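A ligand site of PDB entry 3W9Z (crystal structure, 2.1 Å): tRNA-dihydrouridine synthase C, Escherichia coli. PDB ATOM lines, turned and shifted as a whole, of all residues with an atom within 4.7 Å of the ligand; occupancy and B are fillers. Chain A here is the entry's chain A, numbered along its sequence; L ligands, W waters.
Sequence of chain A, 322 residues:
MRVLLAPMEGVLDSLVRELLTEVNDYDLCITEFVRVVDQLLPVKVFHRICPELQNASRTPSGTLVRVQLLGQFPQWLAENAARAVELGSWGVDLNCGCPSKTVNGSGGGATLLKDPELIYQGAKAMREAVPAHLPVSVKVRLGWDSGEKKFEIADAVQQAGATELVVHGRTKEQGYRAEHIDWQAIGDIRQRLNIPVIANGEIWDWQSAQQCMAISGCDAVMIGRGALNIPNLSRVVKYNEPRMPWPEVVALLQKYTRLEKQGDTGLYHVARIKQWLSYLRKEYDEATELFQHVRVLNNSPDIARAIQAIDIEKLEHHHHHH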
ATOM      1  N   ALA A   6       5.910  -4.199 -27.994  1.00  0.00           N
ATOM      2  CA  ALA A   6       6.254  -2.799 -27.759  1.00  0.00           C
ATOM      3  C   ALA A   6       7.639  -2.640 -27.153  1.00  0.00           C
ATOM      4  O   ALA A   6       8.130  -3.546 -26.498  1.00  0.00           O
ATOM      5  CB  ALA A   6       5.214  -2.135 -26.847  1.00  0.00           C
ATOM      6  N   PRO A   7       8.265  -1.470 -27.372  1.00  0.00           N
ATOM      7  CA  PRO A   7       9.454  -1.122 -26.596  1.00  0.00           C
ATOM      8  C   PRO A   7       9.014  -0.742 -25.176  1.00  0.00           C
ATOM      9  O   PRO A   7       8.029  -0.016 -25.020  1.00  0.00           O
ATOM     10  CB  PRO A   7       9.998   0.099 -27.340  1.00  0.00           C
ATOM     11  CG  PRO A   7       8.769   0.730 -27.997  1.00  0.00           C
ATOM     12  CD  PRO A   7       7.850  -0.412 -28.328  1.00  0.00           C
ATOM     13  N   MET A   8       9.718  -1.255 -24.173  1.00  0.00           N
ATOM     14  CA  MET A   8       9.391  -0.944 -22.787  1.00  0.00           C
ATOM     15  C   MET A   8      10.696  -0.673 -22.068  1.00  0.00           C
ATOM     16  O   MET A   8      11.297  -1.570 -21.478  1.00  0.00           O
ATOM     17  CB  MET A   8       8.678  -2.103 -22.087  1.00  0.00           C
ATOM     18  CG  MET A   8       7.310  -2.443 -22.659  1.00  0.00           C
ATOM     19  SD  MET A   8       6.198  -1.047 -22.643  1.00  0.00           S
ATOM     20  CE  MET A   8       5.538  -1.253 -21.006  1.00  0.00           C
ATOM     21  N   GLU A   9      11.144   0.581 -22.151  1.00  0.00           N
ATOM     22  CA  GLU A   9      12.411   0.953 -21.554  1.00  0.00           C
ATOM     23  C   GLU A   9      12.328   0.772 -20.048  1.00  0.00           C
ATOM     24  O   GLU A   9      11.426   1.304 -19.396  1.00  0.00           O
ATOM     25  CB  GLU A   9      12.747   2.403 -21.885  1.00  0.00           C
ATOM     26  CG  GLU A   9      14.216   2.662 -21.892  1.00  0.00           C
ATOM     27  CD  GLU A   9      14.660   3.405 -20.666  1.00  0.00           C
ATOM     28  OE1 GLU A   9      14.116   4.515 -20.445  1.00  0.00           O
ATOM     29  OE2 GLU A   9      15.547   2.874 -19.959  1.00  0.00           O
ATOM     30  N   VAL A  11      11.881  -2.179 -18.714  1.00  0.00           N
ATOM     31  CA  VAL A  11      11.104  -3.405 -18.474  1.00  0.00           C
ATOM     32  C   VAL A  11      11.563  -4.520 -19.418  1.00  0.00           C
ATOM     33  O   VAL A  11      11.927  -5.592 -18.973  1.00  0.00           O
ATOM     34  CB  VAL A  11       9.568  -3.160 -18.618  1.00  0.00           C
ATOM     35  CG1 VAL A  11       8.800  -4.439 -18.332  1.00  0.00           C
ATOM     36  CG2 VAL A  11       9.098  -2.036 -17.687  1.00  0.00           C
ATOM     37  N   GLU A  32      14.114  -0.880 -26.851  1.00  0.00           N
ATOM     38  CA  GLU A  32      14.099   0.371 -26.111  1.00  0.00           C
ATOM     39  C   GLU A  32      14.877   1.405 -26.935  1.00  0.00           C
ATOM     40  O   GLU A  32      15.782   1.046 -27.710  1.00  0.00           O
ATOM     41  CB  GLU A  32      14.695   0.210 -24.695  1.00  0.00           C
ATOM     42  CG  GLU A  32      16.155  -0.262 -24.635  1.00  0.00           C
ATOM     43  CD  GLU A  32      16.316  -1.780 -24.697  1.00  0.00           C
ATOM     44  OE1 GLU A  32      15.726  -2.400 -25.613  1.00  0.00           O
ATOM     45  OE2 GLU A  32      17.050  -2.356 -23.848  1.00  0.00           O
ATOM     46  N   PHE A  33      14.502   2.665 -26.805  1.00  0.00           N
ATOM     47  CA  PHE A  33      15.066   3.701 -27.662  1.00  0.00           C
ATOM     48  C   PHE A  33      16.535   3.925 -27.429  1.00  0.00           C
ATOM     49  O   PHE A  33      17.028   3.807 -26.307  1.00  0.00           O
ATOM     50  CB  PHE A  33      14.307   5.036 -27.570  1.00  0.00           C
ATOM     51  CG  PHE A  33      14.294   5.642 -26.193  1.00  0.00           C
ATOM     52  CD1 PHE A  33      15.312   6.502 -25.776  1.00  0.00           C
ATOM     53  CD2 PHE A  33      13.243   5.388 -25.321  1.00  0.00           C
ATOM     54  CE1 PHE A  33      15.304   7.051 -24.494  1.00  0.00           C
ATOM     55  CE2 PHE A  33      13.219   5.939 -24.053  1.00  0.00           C
ATOM     56  CZ  PHE A  33      14.247   6.771 -23.636  1.00  0.00           C
ATOM     57  N   GLN A  68      15.033   1.178 -32.230  1.00  0.00           N
ATOM     58  CA  GLN A  68      14.316   2.436 -32.141  1.00  0.00           C
ATOM     59  C   GLN A  68      15.255   3.586 -31.792  1.00  0.00           C
ATOM     60  O   GLN A  68      16.168   3.434 -30.963  1.00  0.00           O
ATOM     61  CB  GLN A  68      13.227   2.353 -31.073  1.00  0.00           C
ATOM     62  CG  GLN A  68      12.402   3.604 -31.013  1.00  0.00           C
ATOM     63  CD  GLN A  68      11.325   3.565 -29.956  1.00  0.00           C
ATOM     64  OE1 GLN A  68      11.607   3.716 -28.760  1.00  0.00           O
ATOM     65  NE2 GLN A  68      10.082   3.399 -30.388  1.00  0.00           N
ATOM     66  N   ASN A  95      10.794   7.113 -32.270  1.00  0.00           N
ATOM     67  CA  ASN A  95       9.915   7.393 -31.141  1.00  0.00           C
ATOM     68  C   ASN A  95       9.465   8.846 -31.155  1.00  0.00           C
ATOM     69  O   ASN A  95      10.277   9.751 -31.060  1.00  0.00           O
ATOM     70  CB  ASN A  95      10.634   7.061 -29.828  1.00  0.00           C
ATOM     71  CG  ASN A  95       9.754   7.243 -28.599  1.00  0.00           C
ATOM     72  OD1 ASN A  95       8.696   7.879 -28.646  1.00  0.00           O
ATOM     73  ND2 ASN A  95      10.189   6.694 -27.482  1.00  0.00           N
ATOM     74  N   CYS A  98       7.013   9.173 -26.545  1.00  0.00           N
ATOM     75  CA  CYS A  98       7.571   9.302 -25.187  1.00  0.00           C
ATOM     76  C   CYS A  98       7.952  10.745 -24.844  1.00  0.00           C
ATOM     77  O   CYS A  98       8.935  10.983 -24.129  1.00  0.00           O
ATOM     78  CB  CYS A  98       8.790   8.386 -24.970  1.00  0.00           C
ATOM     79  SG  CYS A  98       8.462   6.633 -24.563  1.00  0.00           S
ATOM     80  N   LYS A 139       6.440   5.790 -34.260  1.00  0.00           N
ATOM     81  CA  LYS A 139       5.472   5.520 -33.198  1.00  0.00           C
ATOM     82  C   LYS A 139       4.970   6.842 -32.620  1.00  0.00           C
ATOM     83  O   LYS A 139       5.761   7.693 -32.218  1.00  0.00           O
ATOM     84  CB  LYS A 139       6.128   4.649 -32.108  1.00  0.00           C
ATOM     85  CG  LYS A 139       5.182   4.169 -30.989  1.00  0.00           C
ATOM     86  CD  LYS A 139       5.851   3.045 -30.212  1.00  0.00           C
ATOM     87  CE  LYS A 139       5.045   2.634 -29.016  1.00  0.00           C
ATOM     88  NZ  LYS A 139       5.148   3.692 -27.969  1.00  0.00           N
ATOM     89  N   HIS A 168      -0.341   4.963 -30.425  1.00  0.00           N
ATOM     90  CA  HIS A 168      -0.780   4.764 -29.037  1.00  0.00           C
ATOM     91  C   HIS A 168      -2.061   5.589 -28.871  1.00  0.00           C
ATOM     92  O   HIS A 168      -2.031   6.809 -28.949  1.00  0.00           O
ATOM     93  CB  HIS A 168       0.310   5.239 -28.087  1.00  0.00           C
ATOM     94  CG  HIS A 168      -0.022   5.026 -26.639  1.00  0.00           C
ATOM     95  ND1 HIS A 168       0.802   5.478 -25.629  1.00  0.00           N
ATOM     96  CD2 HIS A 168      -1.074   4.434 -26.037  1.00  0.00           C
ATOM     97  CE1 HIS A 168       0.260   5.160 -24.453  1.00  0.00           C
ATOM     98  NE2 HIS A 168      -0.875   4.534 -24.677  1.00  0.00           N
ATOM     99  N   ARG A 170      -3.843   7.284 -27.111  1.00  0.00           N
ATOM    100  CA  ARG A 170      -4.081   8.343 -26.118  1.00  0.00           C
ATOM    101  C   ARG A 170      -3.218   9.546 -26.426  1.00  0.00           C
ATOM    102  O   ARG A 170      -2.133   9.402 -27.019  1.00  0.00           O
ATOM    103  CB  ARG A 170      -3.690   7.905 -24.704  1.00  0.00           C
ATOM    104  CG  ARG A 170      -4.463   6.782 -24.107  1.00  0.00           C
ATOM    105  CD  ARG A 170      -3.469   5.958 -23.330  1.00  0.00           C
ATOM    106  NE  ARG A 170      -4.097   5.114 -22.347  1.00  0.00           N
ATOM    107  CZ  ARG A 170      -3.718   3.870 -22.092  1.00  0.00           C
ATOM    108  NH1 ARG A 170      -2.691   3.320 -22.735  1.00  0.00           N
ATOM    109  NH2 ARG A 170      -4.359   3.187 -21.163  1.00  0.00           N
ATOM    110  N   TYR A 176      -1.554   6.949 -19.211  1.00  0.00           N
ATOM    111  CA  TYR A 176      -1.843   5.533 -19.322  1.00  0.00           C
ATOM    112  C   TYR A 176      -3.203   5.171 -18.744  1.00  0.00           C
ATOM    113  O   TYR A 176      -3.473   4.021 -18.405  1.00  0.00           O
ATOM    114  CB  TYR A 176      -0.717   4.721 -18.659  1.00  0.00           C
ATOM    115  CG  TYR A 176       0.568   4.779 -19.460  1.00  0.00           C
ATOM    116  CD1 TYR A 176       1.409   5.892 -19.375  1.00  0.00           C
ATOM    117  CD2 TYR A 176       0.919   3.754 -20.327  1.00  0.00           C
ATOM    118  CE1 TYR A 176       2.588   5.953 -20.121  1.00  0.00           C
ATOM    119  CE2 TYR A 176       2.082   3.816 -21.089  1.00  0.00           C
ATOM    120  CZ  TYR A 176       2.917   4.913 -20.979  1.00  0.00           C
ATOM    121  OH  TYR A 176       4.062   4.969 -21.729  1.00  0.00           O
ATOM    122  N   ASN A 200      -2.173   0.531 -30.851  1.00  0.00           N
ATOM    123  CA  ASN A 200      -1.521   0.249 -29.594  1.00  0.00           C
ATOM    124  C   ASN A 200      -2.284   0.864 -28.431  1.00  0.00           C
ATOM    125  O   ASN A 200      -2.885   1.954 -28.562  1.00  0.00           O
ATOM    126  CB  ASN A 200      -0.062   0.755 -29.640  1.00  0.00           C
ATOM    127  CG  ASN A 200       0.606   0.799 -28.262  1.00  0.00           C
ATOM    128  OD1 ASN A 200       0.978   1.860 -27.777  1.00  0.00           O
ATOM    129  ND2 ASN A 200       0.783  -0.379 -27.642  1.00  0.00           N
ATOM    130  N   GLY A 201      -2.279   0.170 -27.301  1.00  0.00           N
ATOM    131  CA  GLY A 201      -2.785   0.701 -26.050  1.00  0.00           C
ATOM    132  C   GLY A 201      -3.991  -0.067 -25.532  1.00  0.00           C
ATOM    133  O   GLY A 201      -5.009  -0.155 -26.224  1.00  0.00           O
ATOM    134  N   GLU A 202      -3.843  -0.621 -24.336  1.00  0.00           N
ATOM    135  CA  GLU A 202      -4.921  -1.315 -23.616  1.00  0.00           C
ATOM    136  C   GLU A 202      -5.355  -2.628 -24.279  1.00  0.00           C
ATOM    137  O   GLU A 202      -6.537  -2.982 -24.237  1.00  0.00           O
ATOM    138  CB  GLU A 202      -6.141  -0.417 -23.406  1.00  0.00           C
ATOM    139  CG  GLU A 202      -5.887   0.780 -22.504  1.00  0.00           C
ATOM    140  CD  GLU A 202      -5.456   0.358 -21.098  1.00  0.00           C
ATOM    141  OE1 GLU A 202      -6.068  -0.569 -20.537  1.00  0.00           O
ATOM    142  OE2 GLU A 202      -4.499   0.963 -20.568  1.00  0.00           O
ATOM    143  N   ILE A 203      -4.416  -3.347 -24.904  1.00  0.00           N
ATOM    144  CA  ILE A 203      -4.720  -4.668 -25.445  1.00  0.00           C
ATOM    145  C   ILE A 203      -4.152  -5.671 -24.467  1.00  0.00           C
ATOM    146  O   ILE A 203      -2.932  -5.745 -24.288  1.00  0.00           O
ATOM    147  CB  ILE A 203      -4.086  -4.880 -26.826  1.00  0.00           C
ATOM    148  CG1 ILE A 203      -4.574  -3.823 -27.807  1.00  0.00           C
ATOM    149  CG2 ILE A 203      -4.388  -6.267 -27.340  1.00  0.00           C
ATOM    150  CD1 ILE A 203      -3.892  -3.908 -29.153  1.00  0.00           C
ATOM    151  N   MET A 222       0.196  -3.572 -31.477  1.00  0.00           N
ATOM    152  CA  MET A 222       1.380  -3.646 -30.671  1.00  0.00           C
ATOM    153  C   MET A 222       0.960  -3.784 -29.208  1.00  0.00           C
ATOM    154  O   MET A 222       0.068  -3.076 -28.745  1.00  0.00           O
ATOM    155  CB  MET A 222       2.210  -2.397 -30.881  1.00  0.00           C
ATOM    156  CG  MET A 222       3.352  -2.292 -29.899  1.00  0.00           C
ATOM    157  SD  MET A 222       4.361  -0.817 -30.121  1.00  0.00           S
ATOM    158  CE  MET A 222       5.317  -1.319 -31.538  1.00  0.00           C
ATOM    159  N   ILE A 223       1.614  -4.688 -28.485  1.00  0.00           N
ATOM    160  CA  ILE A 223       1.277  -4.876 -27.075  1.00  0.00           C
ATOM    161  C   ILE A 223       2.490  -4.588 -26.210  1.00  0.00           C
ATOM    162  O   ILE A 223       3.568  -5.088 -26.471  1.00  0.00           O
ATOM    163  CB  ILE A 223       0.743  -6.301 -26.807  1.00  0.00           C
ATOM    164  CG1 ILE A 223       1.629  -7.355 -27.463  1.00  0.00           C
ATOM    165  CG2 ILE A 223      -0.666  -6.483 -27.376  1.00  0.00           C
ATOM    166  CD1 ILE A 223       1.139  -8.786 -27.209  1.00  0.00           C
ATOM    167  N   GLY A 224       2.286  -3.774 -25.185  1.00  0.00           N
ATOM    168  CA  GLY A 224       3.368  -3.472 -24.265  1.00  0.00           C
ATOM    169  C   GLY A 224       3.179  -4.143 -22.920  1.00  0.00           C
ATOM    170  O   GLY A 224       3.623  -5.276 -22.721  1.00  0.00           O
ATOM    171  N   ARG A 225       2.515  -3.434 -22.012  1.00  0.00           N
ATOM    172  CA  ARG A 225       2.433  -3.871 -20.623  1.00  0.00           C
ATOM    173  C   ARG A 225       1.804  -5.259 -20.519  1.00  0.00           C
ATOM    174  O   ARG A 225       2.254  -6.089 -19.736  1.00  0.00           O
ATOM    175  CB  ARG A 225       1.676  -2.857 -19.773  1.00  0.00           C
ATOM    176  CG  ARG A 225       2.320  -1.481 -19.696  1.00  0.00           C
ATOM    177  CD  ARG A 225       1.359  -0.456 -19.132  1.00  0.00           C
ATOM    178  NE  ARG A 225       0.264  -0.162 -20.059  1.00  0.00           N
ATOM    179  CZ  ARG A 225      -0.891   0.391 -19.686  1.00  0.00           C
ATOM    180  NH1 ARG A 225      -1.104   0.679 -18.424  1.00  0.00           N
ATOM    181  NH2 ARG A 225      -1.834   0.637 -20.588  1.00  0.00           N
ATOM    182  N   GLY A 226       0.786  -5.505 -21.347  1.00  0.00           N
ATOM    183  CA  GLY A 226       0.108  -6.797 -21.374  1.00  0.00           C
ATOM    184  C   GLY A 226       1.002  -7.985 -21.655  1.00  0.00           C
ATOM    185  O   GLY A 226       0.717  -9.100 -21.213  1.00  0.00           O
ATOM    186  N   TYR A 279       4.074  -7.177 -12.218  1.00  0.00           N
ATOM    187  CA  TYR A 279       3.150  -7.152 -13.351  1.00  0.00           C
ATOM    188  C   TYR A 279       2.214  -8.367 -13.314  1.00  0.00           C
ATOM    189  O   TYR A 279       1.014  -8.249 -13.524  1.00  0.00           O
ATOM    190  CB  TYR A 279       3.926  -7.129 -14.671  1.00  0.00           C
ATOM    191  CG  TYR A 279       4.298  -5.743 -15.162  1.00  0.00           C
ATOM    192  CD1 TYR A 279       3.476  -5.080 -16.081  1.00  0.00           C
ATOM    193  CD2 TYR A 279       5.457  -5.098 -14.728  1.00  0.00           C
ATOM    194  CE1 TYR A 279       3.799  -3.817 -16.542  1.00  0.00           C
ATOM    195  CE2 TYR A 279       5.779  -3.822 -15.192  1.00  0.00           C
ATOM    196  CZ  TYR A 279       4.949  -3.193 -16.098  1.00  0.00           C
ATOM    197  OH  TYR A 279       5.243  -1.923 -16.573  1.00  0.00           O
HETATM  198  N1  LIG L   1       7.395   3.681 -26.138  1.00  0.00           N
HETATM  199  C1  LIG L   1       8.441   3.862 -27.029  1.00  0.00           C
HETATM  200  O1  LIG L   1       8.206   4.227 -28.176  1.00  0.00           O
HETATM  201  N2  LIG L   1       9.743   3.616 -26.635  1.00  0.00           N
HETATM  202  C2  LIG L   1      10.012   3.203 -25.337  1.00  0.00           C
HETATM  203  O2  LIG L   1      11.172   2.998 -24.998  1.00  0.00           O
HETATM  204  C3  LIG L   1       8.953   3.028 -24.445  1.00  0.00           C
HETATM  205  N3  LIG L   1       9.187   2.623 -23.155  1.00  0.00           N
HETATM  206  C4  LIG L   1       8.130   2.439 -22.273  1.00  0.00           C
HETATM  207  C5  LIG L   1       8.401   2.012 -20.972  1.00  0.00           C
HETATM  208  C6  LIG L   1       7.372   1.817 -20.061  1.00  0.00           C
HETATM  209  C7  LIG L   1       7.702   1.367 -18.660  1.00  0.00           C
HETATM  210  C8  LIG L   1       6.062   2.042 -20.447  1.00  0.00           C
HETATM  211  C9  LIG L   1       4.941   1.823 -19.453  1.00  0.00           C
HETATM  212  C10 LIG L   1       5.783   2.455 -21.767  1.00  0.00           C
HETATM  213  C11 LIG L   1       6.822   2.657 -22.682  1.00  0.00           C
HETATM  214  N4  LIG L   1       6.575   3.086 -23.989  1.00  0.00           N
HETATM  215  C12 LIG L   1       7.644   3.260 -24.859  1.00  0.00           C
HETATM  216  C13 LIG L   1       5.179   3.299 -24.507  1.00  0.00           C
HETATM  217  C14 LIG L   1       4.707   1.848 -24.864  1.00  0.00           C
HETATM  218  O3  LIG L   1       5.540   1.219 -25.823  1.00  0.00           O
HETATM  219  C15 LIG L   1       3.253   1.685 -25.300  1.00  0.00           C
HETATM  220  O4  LIG L   1       2.930   2.557 -26.371  1.00  0.00           O
HETATM  221  C16 LIG L   1       2.318   1.903 -24.102  1.00  0.00           C
HETATM  222  O5  LIG L   1       2.722   1.084 -23.034  1.00  0.00           O
HETATM  223  C17 LIG L   1       0.868   1.588 -24.452  1.00  0.00           C
HETATM  224  O6  LIG L   1       0.747   0.229 -24.818  1.00  0.00           O
HETATM  225  P1  LIG L   1       0.134  -0.870 -23.775  1.00  0.00           P
HETATM  226  O7  LIG L   1      -1.198  -0.375 -23.295  1.00  0.00           O
HETATM  227  O8  LIG L   1       1.125  -1.067 -22.645  1.00  0.00           O
HETATM  228  O9  LIG L   1      -0.041  -2.188 -24.513  1.00  0.00           O
HETATM  229  O   HOH W   1       4.442   2.981 -16.248  1.00  0.00           O
HETATM  230  O   HOH W   2      -0.601  -4.484 -23.579  1.00  0.00           O
HETATM  231  O   HOH W   3      -1.642  -2.524 -26.427  1.00  0.00           O
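Water W2 lies within hydrogen-bond range of an oxygen (O9) of the ligand, the backbone carbonyl oxygen (O) of Ile 203, the backbone NH (N) of Gly 226 and the backbone NH (N) of Gly 224.
Ala 6 touches the ligand (CB to O3, 3.5 Å).
CE of Met 8 touches C8 of the ligand, 3.4 Å away.
Val 11 touches the ligand.
CD2 of Phe 33 touches O2 of the ligand (3.2 Å).
His 168 touches the ligand (NE2 to C17, 3.4 Å).
OH of Tyr 176 touches C10 of the ligand (3.0 Å).
Gly 201 touches the ligand.
C of Ile 223 touches O9 of the ligand, 3.9 Å away.
Hydrophobic or aromatic side chains that line the ligand: Ala 6, Pro 7, Met 8, Val 11, Phe 33, His 168 and Tyr 176.
Within 4 Å of the ligand: Ala 6, Pro 7, Met 8, Glu 9, Val 11, Phe 33, Gln 68, Asn 95, Cys 98, Lys 139, His 168, Tyr 176, Asn 200, Gly 201, Glu 202, Ile 223, Gly 224 and Arg 225.
Along chain A the residues within 4 Å of the ligand span positions 6 to 225.
The nearest printed residue that does not touch the ligand is Arg 170 (4.02 Å).
The side-chain carboxylate (OE2) of Glu 202 lies within salt-bridge range of the guanidinium group (NH2) of Arg 225, at 2.7 Å.
The backbone NH of Ala 6 lies within hydrogen-bond range of the backbone carbonyl oxygen of Ile 223.
A ring nitrogen (NE2) of His 168 sits at hydrogen-bond distance from the guanidinium group (NH1) of Arg 170.
The side-chain amide oxygen (OD1) of Asn 95 sits at hydrogen-bond distance from the backbone NH (N) of Cys 98.
NH1 of Arg 170 lies within salt-bridge range of OE2 of Glu 202 (3.7 Å).
O of Tyr 176 sits at hydrogen-bond distance from NH2 of Arg 170.
ND2 of Asn 200 lies within hydrogen-bond range of O of Met 222 (3.0 Å).
N of Glu 202 sits at hydrogen-bond distance from O7 of the ligand (2.9 Å).
The side-chain amino group of Lys 139 sits at hydrogen-bond distance from a nitrogen (N1) of the ligand.
The side-chain amide oxygen (OD1) of Asn 200 is in hydrogen-bond range of an oxygen (O4) of the ligand.
The backbone carbonyl oxygen of Pro 7 lies within hydrogen-bond range of an oxygen (O3) of the ligand, at 2.9 Å.
OE1 of Gln 68 is in hydrogen-bond range of N2 of the ligand.
N1 of the ligand sits close to SG of Cys 98 (3.5 Å).
The side-chain amide nitrogen (ND2) of Asn 95 sits close to a nitrogen (N2) of the ligand (3.2 Å).
The guanidinium group of Arg 225 lies within salt-bridge range of an oxygen (O8) of the ligand, 2.9 Å away.
The backbone NH of Arg 225 is in hydrogen-bond range of an oxygen (O8) of the ligand (2.8 Å).
N of Glu 9 lies within hydrogen-bond range of N3 of the ligand (3.0 Å).
O9 of the ligand is in hydrogen-bond range of N of Gly 224.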
